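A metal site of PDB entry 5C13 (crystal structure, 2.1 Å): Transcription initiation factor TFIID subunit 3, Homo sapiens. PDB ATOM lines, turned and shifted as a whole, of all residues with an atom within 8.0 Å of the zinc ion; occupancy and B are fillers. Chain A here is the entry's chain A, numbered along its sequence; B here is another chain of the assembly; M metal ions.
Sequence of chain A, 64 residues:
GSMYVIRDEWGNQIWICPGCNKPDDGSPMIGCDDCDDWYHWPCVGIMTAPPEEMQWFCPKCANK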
ATOM      1  N   ILE A  16     -27.420  10.401   9.893  1.00  0.00           N
ATOM      2  CA  ILE A  16     -27.940  11.203  10.996  1.00  0.00           C
ATOM      3  C   ILE A  16     -26.932  11.333  12.144  1.00  0.00           C
ATOM      4  O   ILE A  16     -26.433  10.327  12.651  1.00  0.00           O
ATOM      5  CB  ILE A  16     -29.256  10.587  11.571  1.00  0.00           C
ATOM      6  CG1 ILE A  16     -30.244  10.230  10.437  1.00  0.00           C
ATOM      7  CG2 ILE A  16     -29.865  11.497  12.578  1.00  0.00           C
ATOM      8  CD1 ILE A  16     -30.744  11.398   9.696  1.00  0.00           C
ATOM      9  N   CYS A  17     -26.673  12.575  12.563  1.00  0.00           N
ATOM     10  CA  CYS A  17     -25.986  12.846  13.832  1.00  0.00           C
ATOM     11  C   CYS A  17     -26.567  12.036  14.990  1.00  0.00           C
ATOM     12  O   CYS A  17     -27.751  12.158  15.285  1.00  0.00           O
ATOM     13  CB  CYS A  17     -26.088  14.333  14.139  1.00  0.00           C
ATOM     14  SG  CYS A  17     -25.526  14.874  15.710  1.00  0.00           S
ATOM     15  N   PRO A  18     -25.757  11.190  15.651  1.00  0.00           N
ATOM     16  CA  PRO A  18     -26.305  10.456  16.807  1.00  0.00           C
ATOM     17  C   PRO A  18     -26.565  11.369  18.045  1.00  0.00           C
ATOM     18  O   PRO A  18     -27.195  10.969  19.004  1.00  0.00           O
ATOM     19  CB  PRO A  18     -25.221   9.424  17.130  1.00  0.00           C
ATOM     20  CG  PRO A  18     -24.276   9.417  15.989  1.00  0.00           C
ATOM     21  CD  PRO A  18     -24.364  10.771  15.348  1.00  0.00           C
ATOM     22  N   GLY A  19     -26.078  12.601  18.007  1.00  0.00           N
ATOM     23  CA  GLY A  19     -26.266  13.487  19.136  1.00  0.00           C
ATOM     24  C   GLY A  19     -27.679  13.997  19.235  1.00  0.00           C
ATOM     25  O   GLY A  19     -28.286  14.017  20.304  1.00  0.00           O
ATOM     26  N   CYS A  20     -28.205  14.439  18.110  1.00  0.00           N
ATOM     27  CA  CYS A  20     -29.546  14.965  18.099  1.00  0.00           C
ATOM     28  C   CYS A  20     -30.532  14.000  17.386  1.00  0.00           C
ATOM     29  O   CYS A  20     -31.730  14.011  17.662  1.00  0.00           O
ATOM     30  CB  CYS A  20     -29.504  16.332  17.423  1.00  0.00           C
ATOM     31  SG  CYS A  20     -29.059  16.273  15.675  1.00  0.00           S
ATOM     32  N   ASN A  21     -29.998  13.169  16.489  1.00  0.00           N
ATOM     33  CA  ASN A  21     -30.820  12.274  15.655  1.00  0.00           C
ATOM     34  C   ASN A  21     -31.888  13.052  14.914  1.00  0.00           C
ATOM     35  O   ASN A  21     -32.999  12.578  14.721  1.00  0.00           O
ATOM     36  CB  ASN A  21     -31.424  11.142  16.490  1.00  0.00           C
ATOM     37  CG  ASN A  21     -30.528   9.929  16.569  1.00  0.00           C
ATOM     38  OD1 ASN A  21     -30.147   9.385  15.549  1.00  0.00           O
ATOM     39  ND2 ASN A  21     -30.189   9.495  17.780  1.00  0.00           N
ATOM     40  N   LYS A  22     -31.540  14.269  14.508  1.00  0.00           N
ATOM     41  CA  LYS A  22     -32.371  15.057  13.636  1.00  0.00           C
ATOM     42  C   LYS A  22     -31.691  15.066  12.259  1.00  0.00           C
ATOM     43  O   LYS A  22     -30.484  15.332  12.145  1.00  0.00           O
ATOM     44  CB  LYS A  22     -32.596  16.478  14.169  1.00  0.00           C
ATOM     45  CG  LYS A  22     -33.489  16.544  15.414  1.00  0.00           C
ATOM     46  CD  LYS A  22     -34.934  16.940  15.111  1.00  0.00           C
ATOM     47  CE  LYS A  22     -35.417  18.076  15.997  1.00  0.00           C
ATOM     48  NZ  LYS A  22     -36.869  18.352  15.759  1.00  0.00           N
ATOM     49  N   PRO A  23     -32.444  14.717  11.221  1.00  0.00           N
ATOM     50  CA  PRO A  23     -31.870  14.816   9.877  1.00  0.00           C
ATOM     51  C   PRO A  23     -31.657  16.232   9.362  1.00  0.00           C
ATOM     52  O   PRO A  23     -30.799  16.425   8.507  1.00  0.00           O
ATOM     53  CB  PRO A  23     -32.916  14.108   9.017  1.00  0.00           C
ATOM     54  CG  PRO A  23     -34.159  14.129   9.825  1.00  0.00           C
ATOM     55  CD  PRO A  23     -33.730  14.022  11.229  1.00  0.00           C
ATOM     56  N   ASP A  24     -32.417  17.200   9.838  1.00  0.00           N
ATOM     57  CA  ASP A  24     -32.323  18.511   9.217  1.00  0.00           C
ATOM     58  C   ASP A  24     -31.174  19.312   9.788  1.00  0.00           C
ATOM     59  O   ASP A  24     -31.287  19.950  10.837  1.00  0.00           O
ATOM     60  CB  ASP A  24     -33.643  19.255   9.359  1.00  0.00           C
ATOM     61  CG  ASP A  24     -34.684  18.729   8.399  1.00  0.00           C
ATOM     62  OD1 ASP A  24     -34.291  18.189   7.336  1.00  0.00           O
ATOM     63  OD2 ASP A  24     -35.884  18.856   8.695  1.00  0.00           O
ATOM     64  N   ASP A  25     -30.059  19.265   9.078  1.00  0.00           N
ATOM     65  CA  ASP A  25     -28.837  19.924   9.505  1.00  0.00           C
ATOM     66  C   ASP A  25     -28.780  21.337   9.019  1.00  0.00           C
ATOM     67  O   ASP A  25     -29.384  22.242   9.608  1.00  0.00           O
ATOM     68  CB  ASP A  25     -27.601  19.176   8.992  1.00  0.00           C
ATOM     69  CG  ASP A  25     -27.724  17.690   9.141  1.00  0.00           C
ATOM     70  OD1 ASP A  25     -28.383  17.268  10.109  1.00  0.00           O
ATOM     71  OD2 ASP A  25     -27.143  16.948   8.325  1.00  0.00           O
ATOM     72  N   SER A  27     -26.155  22.644   9.646  1.00  0.00           N
ATOM     73  CA  SER A  27     -24.996  22.650  10.519  1.00  0.00           C
ATOM     74  C   SER A  27     -23.838  21.694  10.145  1.00  0.00           C
ATOM     75  O   SER A  27     -24.061  20.516   9.844  1.00  0.00           O
ATOM     76  CB  SER A  27     -25.471  22.320  11.931  1.00  0.00           C
ATOM     77  OG  SER A  27     -24.350  22.038  12.736  1.00  0.00           O
ATOM     78  N   PRO A  28     -22.603  22.201  10.183  1.00  0.00           N
ATOM     79  CA  PRO A  28     -21.445  21.393   9.801  1.00  0.00           C
ATOM     80  C   PRO A  28     -21.279  20.191  10.693  1.00  0.00           C
ATOM     81  O   PRO A  28     -21.776  20.227  11.834  1.00  0.00           O
ATOM     82  CB  PRO A  28     -20.274  22.353   9.967  1.00  0.00           C
ATOM     83  CG  PRO A  28     -20.745  23.322  10.974  1.00  0.00           C
ATOM     84  CD  PRO A  28     -22.189  23.507  10.701  1.00  0.00           C
ATOM     85  N   MET A  29     -20.618  19.157  10.180  1.00  0.00           N
ATOM     86  CA  MET A  29     -20.334  17.945  10.952  1.00  0.00           C
ATOM     87  C   MET A  29     -18.864  17.601  11.077  1.00  0.00           C
ATOM     88  O   MET A  29     -18.028  18.062  10.299  1.00  0.00           O
ATOM     89  CB  MET A  29     -21.056  16.775  10.321  1.00  0.00           C
ATOM     90  CG  MET A  29     -22.572  17.018  10.235  1.00  0.00           C
ATOM     91  SD  MET A  29     -23.473  15.692   9.428  1.00  0.00           S
ATOM     92  CE  MET A  29     -23.906  14.615  10.765  1.00  0.00           C
ATOM     93  N   TRP A  38     -20.346  10.483  12.570  1.00  0.00           N
ATOM     94  CA  TRP A  38     -20.283  11.917  12.367  1.00  0.00           C
ATOM     95  C   TRP A  38     -21.338  12.662  13.184  1.00  0.00           C
ATOM     96  O   TRP A  38     -22.467  12.179  13.310  1.00  0.00           O
ATOM     97  CB  TRP A  38     -20.452  12.233  10.887  1.00  0.00           C
ATOM     98  CG  TRP A  38     -19.275  11.776  10.035  1.00  0.00           C
ATOM     99  CD1 TRP A  38     -18.908  10.487   9.799  1.00  0.00           C
ATOM    100  CD2 TRP A  38     -18.325  12.604   9.334  1.00  0.00           C
ATOM    101  NE1 TRP A  38     -17.779  10.468   8.974  1.00  0.00           N
ATOM    102  CE2 TRP A  38     -17.426  11.750   8.688  1.00  0.00           C
ATOM    103  CE3 TRP A  38     -18.172  13.984   9.177  1.00  0.00           C
ATOM    104  CZ2 TRP A  38     -16.363  12.227   7.906  1.00  0.00           C
ATOM    105  CZ3 TRP A  38     -17.126  14.444   8.417  1.00  0.00           C
ATOM    106  CH2 TRP A  38     -16.239  13.565   7.793  1.00  0.00           C
ATOM    107  N   TYR A  39     -20.970  13.824  13.726  1.00  0.00           N
ATOM    108  CA  TYR A  39     -21.863  14.625  14.577  1.00  0.00           C
ATOM    109  C   TYR A  39     -21.869  16.027  14.087  1.00  0.00           C
ATOM    110  O   TYR A  39     -20.879  16.486  13.549  1.00  0.00           O
ATOM    111  CB  TYR A  39     -21.387  14.650  16.048  1.00  0.00           C
ATOM    112  CG  TYR A  39     -21.494  13.375  16.804  1.00  0.00           C
ATOM    113  CD1 TYR A  39     -20.682  12.285  16.525  1.00  0.00           C
ATOM    114  CD2 TYR A  39     -22.389  13.272  17.859  1.00  0.00           C
ATOM    115  CE1 TYR A  39     -20.796  11.093  17.260  1.00  0.00           C
ATOM    116  CE2 TYR A  39     -22.487  12.118  18.607  1.00  0.00           C
ATOM    117  CZ  TYR A  39     -21.726  11.021  18.295  1.00  0.00           C
ATOM    118  OH  TYR A  39     -21.889   9.885  19.074  1.00  0.00           O
ATOM    119  N   HIS A  40     -22.952  16.747  14.303  1.00  0.00           N
ATOM    120  CA  HIS A  40     -22.914  18.203  14.208  1.00  0.00           C
ATOM    121  C   HIS A  40     -21.993  18.802  15.251  1.00  0.00           C
ATOM    122  O   HIS A  40     -22.005  18.382  16.422  1.00  0.00           O
ATOM    123  CB  HIS A  40     -24.297  18.817  14.431  1.00  0.00           C
ATOM    124  CG  HIS A  40     -25.372  18.257  13.579  1.00  0.00           C
ATOM    125  ND1 HIS A  40     -26.477  17.610  14.095  1.00  0.00           N
ATOM    126  CD2 HIS A  40     -25.549  18.294  12.235  1.00  0.00           C
ATOM    127  CE1 HIS A  40     -27.275  17.244  13.108  1.00  0.00           C
ATOM    128  NE2 HIS A  40     -26.730  17.649  11.969  1.00  0.00           N
ATOM    129  N   TRP A  41     -21.237  19.814  14.820  1.00  0.00           N
ATOM    130  CA  TRP A  41     -20.394  20.610  15.682  1.00  0.00           C
ATOM    131  C   TRP A  41     -21.056  20.989  16.992  1.00  0.00           C
ATOM    132  O   TRP A  41     -20.490  20.742  18.036  1.00  0.00           O
ATOM    133  CB  TRP A  41     -19.932  21.860  14.938  1.00  0.00           C
ATOM    134  CG  TRP A  41     -18.956  21.536  13.846  1.00  0.00           C
ATOM    135  CD1 TRP A  41     -18.731  20.328  13.284  1.00  0.00           C
ATOM    136  CD2 TRP A  41     -18.067  22.459  13.190  1.00  0.00           C
ATOM    137  NE1 TRP A  41     -17.745  20.419  12.317  1.00  0.00           N
ATOM    138  CE2 TRP A  41     -17.339  21.728  12.233  1.00  0.00           C
ATOM    139  CE3 TRP A  41     -17.822  23.827  13.312  1.00  0.00           C
ATOM    140  CZ2 TRP A  41     -16.376  22.308  11.413  1.00  0.00           C
ATOM    141  CZ3 TRP A  41     -16.882  24.409  12.485  1.00  0.00           C
ATOM    142  CH2 TRP A  41     -16.159  23.655  11.557  1.00  0.00           C
ATOM    143  N   PRO A  42     -22.254  21.596  16.952  1.00  0.00           N
ATOM    144  CA  PRO A  42     -22.828  22.039  18.222  1.00  0.00           C
ATOM    145  C   PRO A  42     -23.291  20.871  19.086  1.00  0.00           C
ATOM    146  O   PRO A  42     -23.360  21.004  20.299  1.00  0.00           O
ATOM    147  CB  PRO A  42     -24.011  22.911  17.791  1.00  0.00           C
ATOM    148  CG  PRO A  42     -24.277  22.556  16.397  1.00  0.00           C
ATOM    149  CD  PRO A  42     -22.961  22.187  15.814  1.00  0.00           C
ATOM    150  N   CYS A  43     -23.582  19.737  18.470  1.00  0.00           N
ATOM    151  CA  CYS A  43     -24.001  18.585  19.254  1.00  0.00           C
ATOM    152  C   CYS A  43     -22.835  18.022  20.024  1.00  0.00           C
ATOM    153  O   CYS A  43     -23.057  17.267  20.952  1.00  0.00           O
ATOM    154  CB  CYS A  43     -24.637  17.513  18.349  1.00  0.00           C
ATOM    155  SG  CYS A  43     -26.146  18.114  17.595  1.00  0.00           S
ATOM    156  N   VAL A  44     -21.603  18.395  19.681  1.00  0.00           N
ATOM    157  CA  VAL A  44     -20.469  17.905  20.459  1.00  0.00           C
ATOM    158  C   VAL A  44     -19.638  19.039  21.050  1.00  0.00           C
ATOM    159  O   VAL A  44     -18.526  18.799  21.509  1.00  0.00           O
ATOM    160  CB  VAL A  44     -19.557  16.962  19.608  1.00  0.00           C
ATOM    161  CG1 VAL A  44     -20.218  15.630  19.371  1.00  0.00           C
ATOM    162  CG2 VAL A  44     -19.144  17.609  18.282  1.00  0.00           C
ATOM    163  N   ASN B  12     -26.704  12.114  24.397  1.00  0.00           N
ATOM    164  CA  ASN B  12     -27.375  11.923  23.113  1.00  0.00           C
ATOM    165  C   ASN B  12     -28.882  11.700  23.227  1.00  0.00           C
ATOM    166  O   ASN B  12     -29.382  11.122  24.188  1.00  0.00           O
ATOM    167  CB  ASN B  12     -26.794  10.725  22.385  1.00  0.00           C
ATOM    168  CG  ASN B  12     -25.394  10.967  21.914  1.00  0.00           C
ATOM    169  OD1 ASN B  12     -24.937  12.104  21.794  1.00  0.00           O
ATOM    170  ND2 ASN B  12     -24.681   9.885  21.647  1.00  0.00           N
ATOM    171  N   GLN B  13     -29.581  12.112  22.174  1.00  0.00           N
ATOM    172  CA  GLN B  13     -31.038  12.046  22.122  1.00  0.00           C
ATOM    173  C   GLN B  13     -31.556  10.908  21.297  1.00  0.00           C
ATOM    174  O   GLN B  13     -31.238  10.799  20.115  1.00  0.00           O
ATOM    175  CB  GLN B  13     -31.584  13.323  21.538  1.00  0.00           C
ATOM    176  CG  GLN B  13     -31.604  14.451  22.481  1.00  0.00           C
ATOM    177  CD  GLN B  13     -32.171  15.647  21.785  1.00  0.00           C
ATOM    178  OE1 GLN B  13     -32.514  15.582  20.605  1.00  0.00           O
ATOM    179  NE2 GLN B  13     -32.276  16.748  22.498  1.00  0.00           N
HETATM  180 ZN    ZN M   1     -26.755  16.688  15.898  1.00  0.00          ZN
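The side-chain carboxylate of Asp 25 is in hydrogen-bond range of a ring nitrogen (NE2) of His 40, 2.5 Å away.
The backbone NH of Gly 19 lies close to the side-chain sulfur of Cys 17 (3.3 Å).
SG of Cys 20 sits close to N of Lys 22, 3.4 Å away.
O of Cys 20 lies close to OE1 of Gln 13 of chain B, 3.4 Å away.
Four residues have an atom within 4 Å of the zinc ion: Cys 17, Cys 20, His 40 and Cys 43.
The zinc ion is bound by ND1 of His 40 (2.0 Å), SG of Cys 17 (2.2 Å), SG of Cys 43 (2.3 Å) and SG of Cys 20 (2.4 Å).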
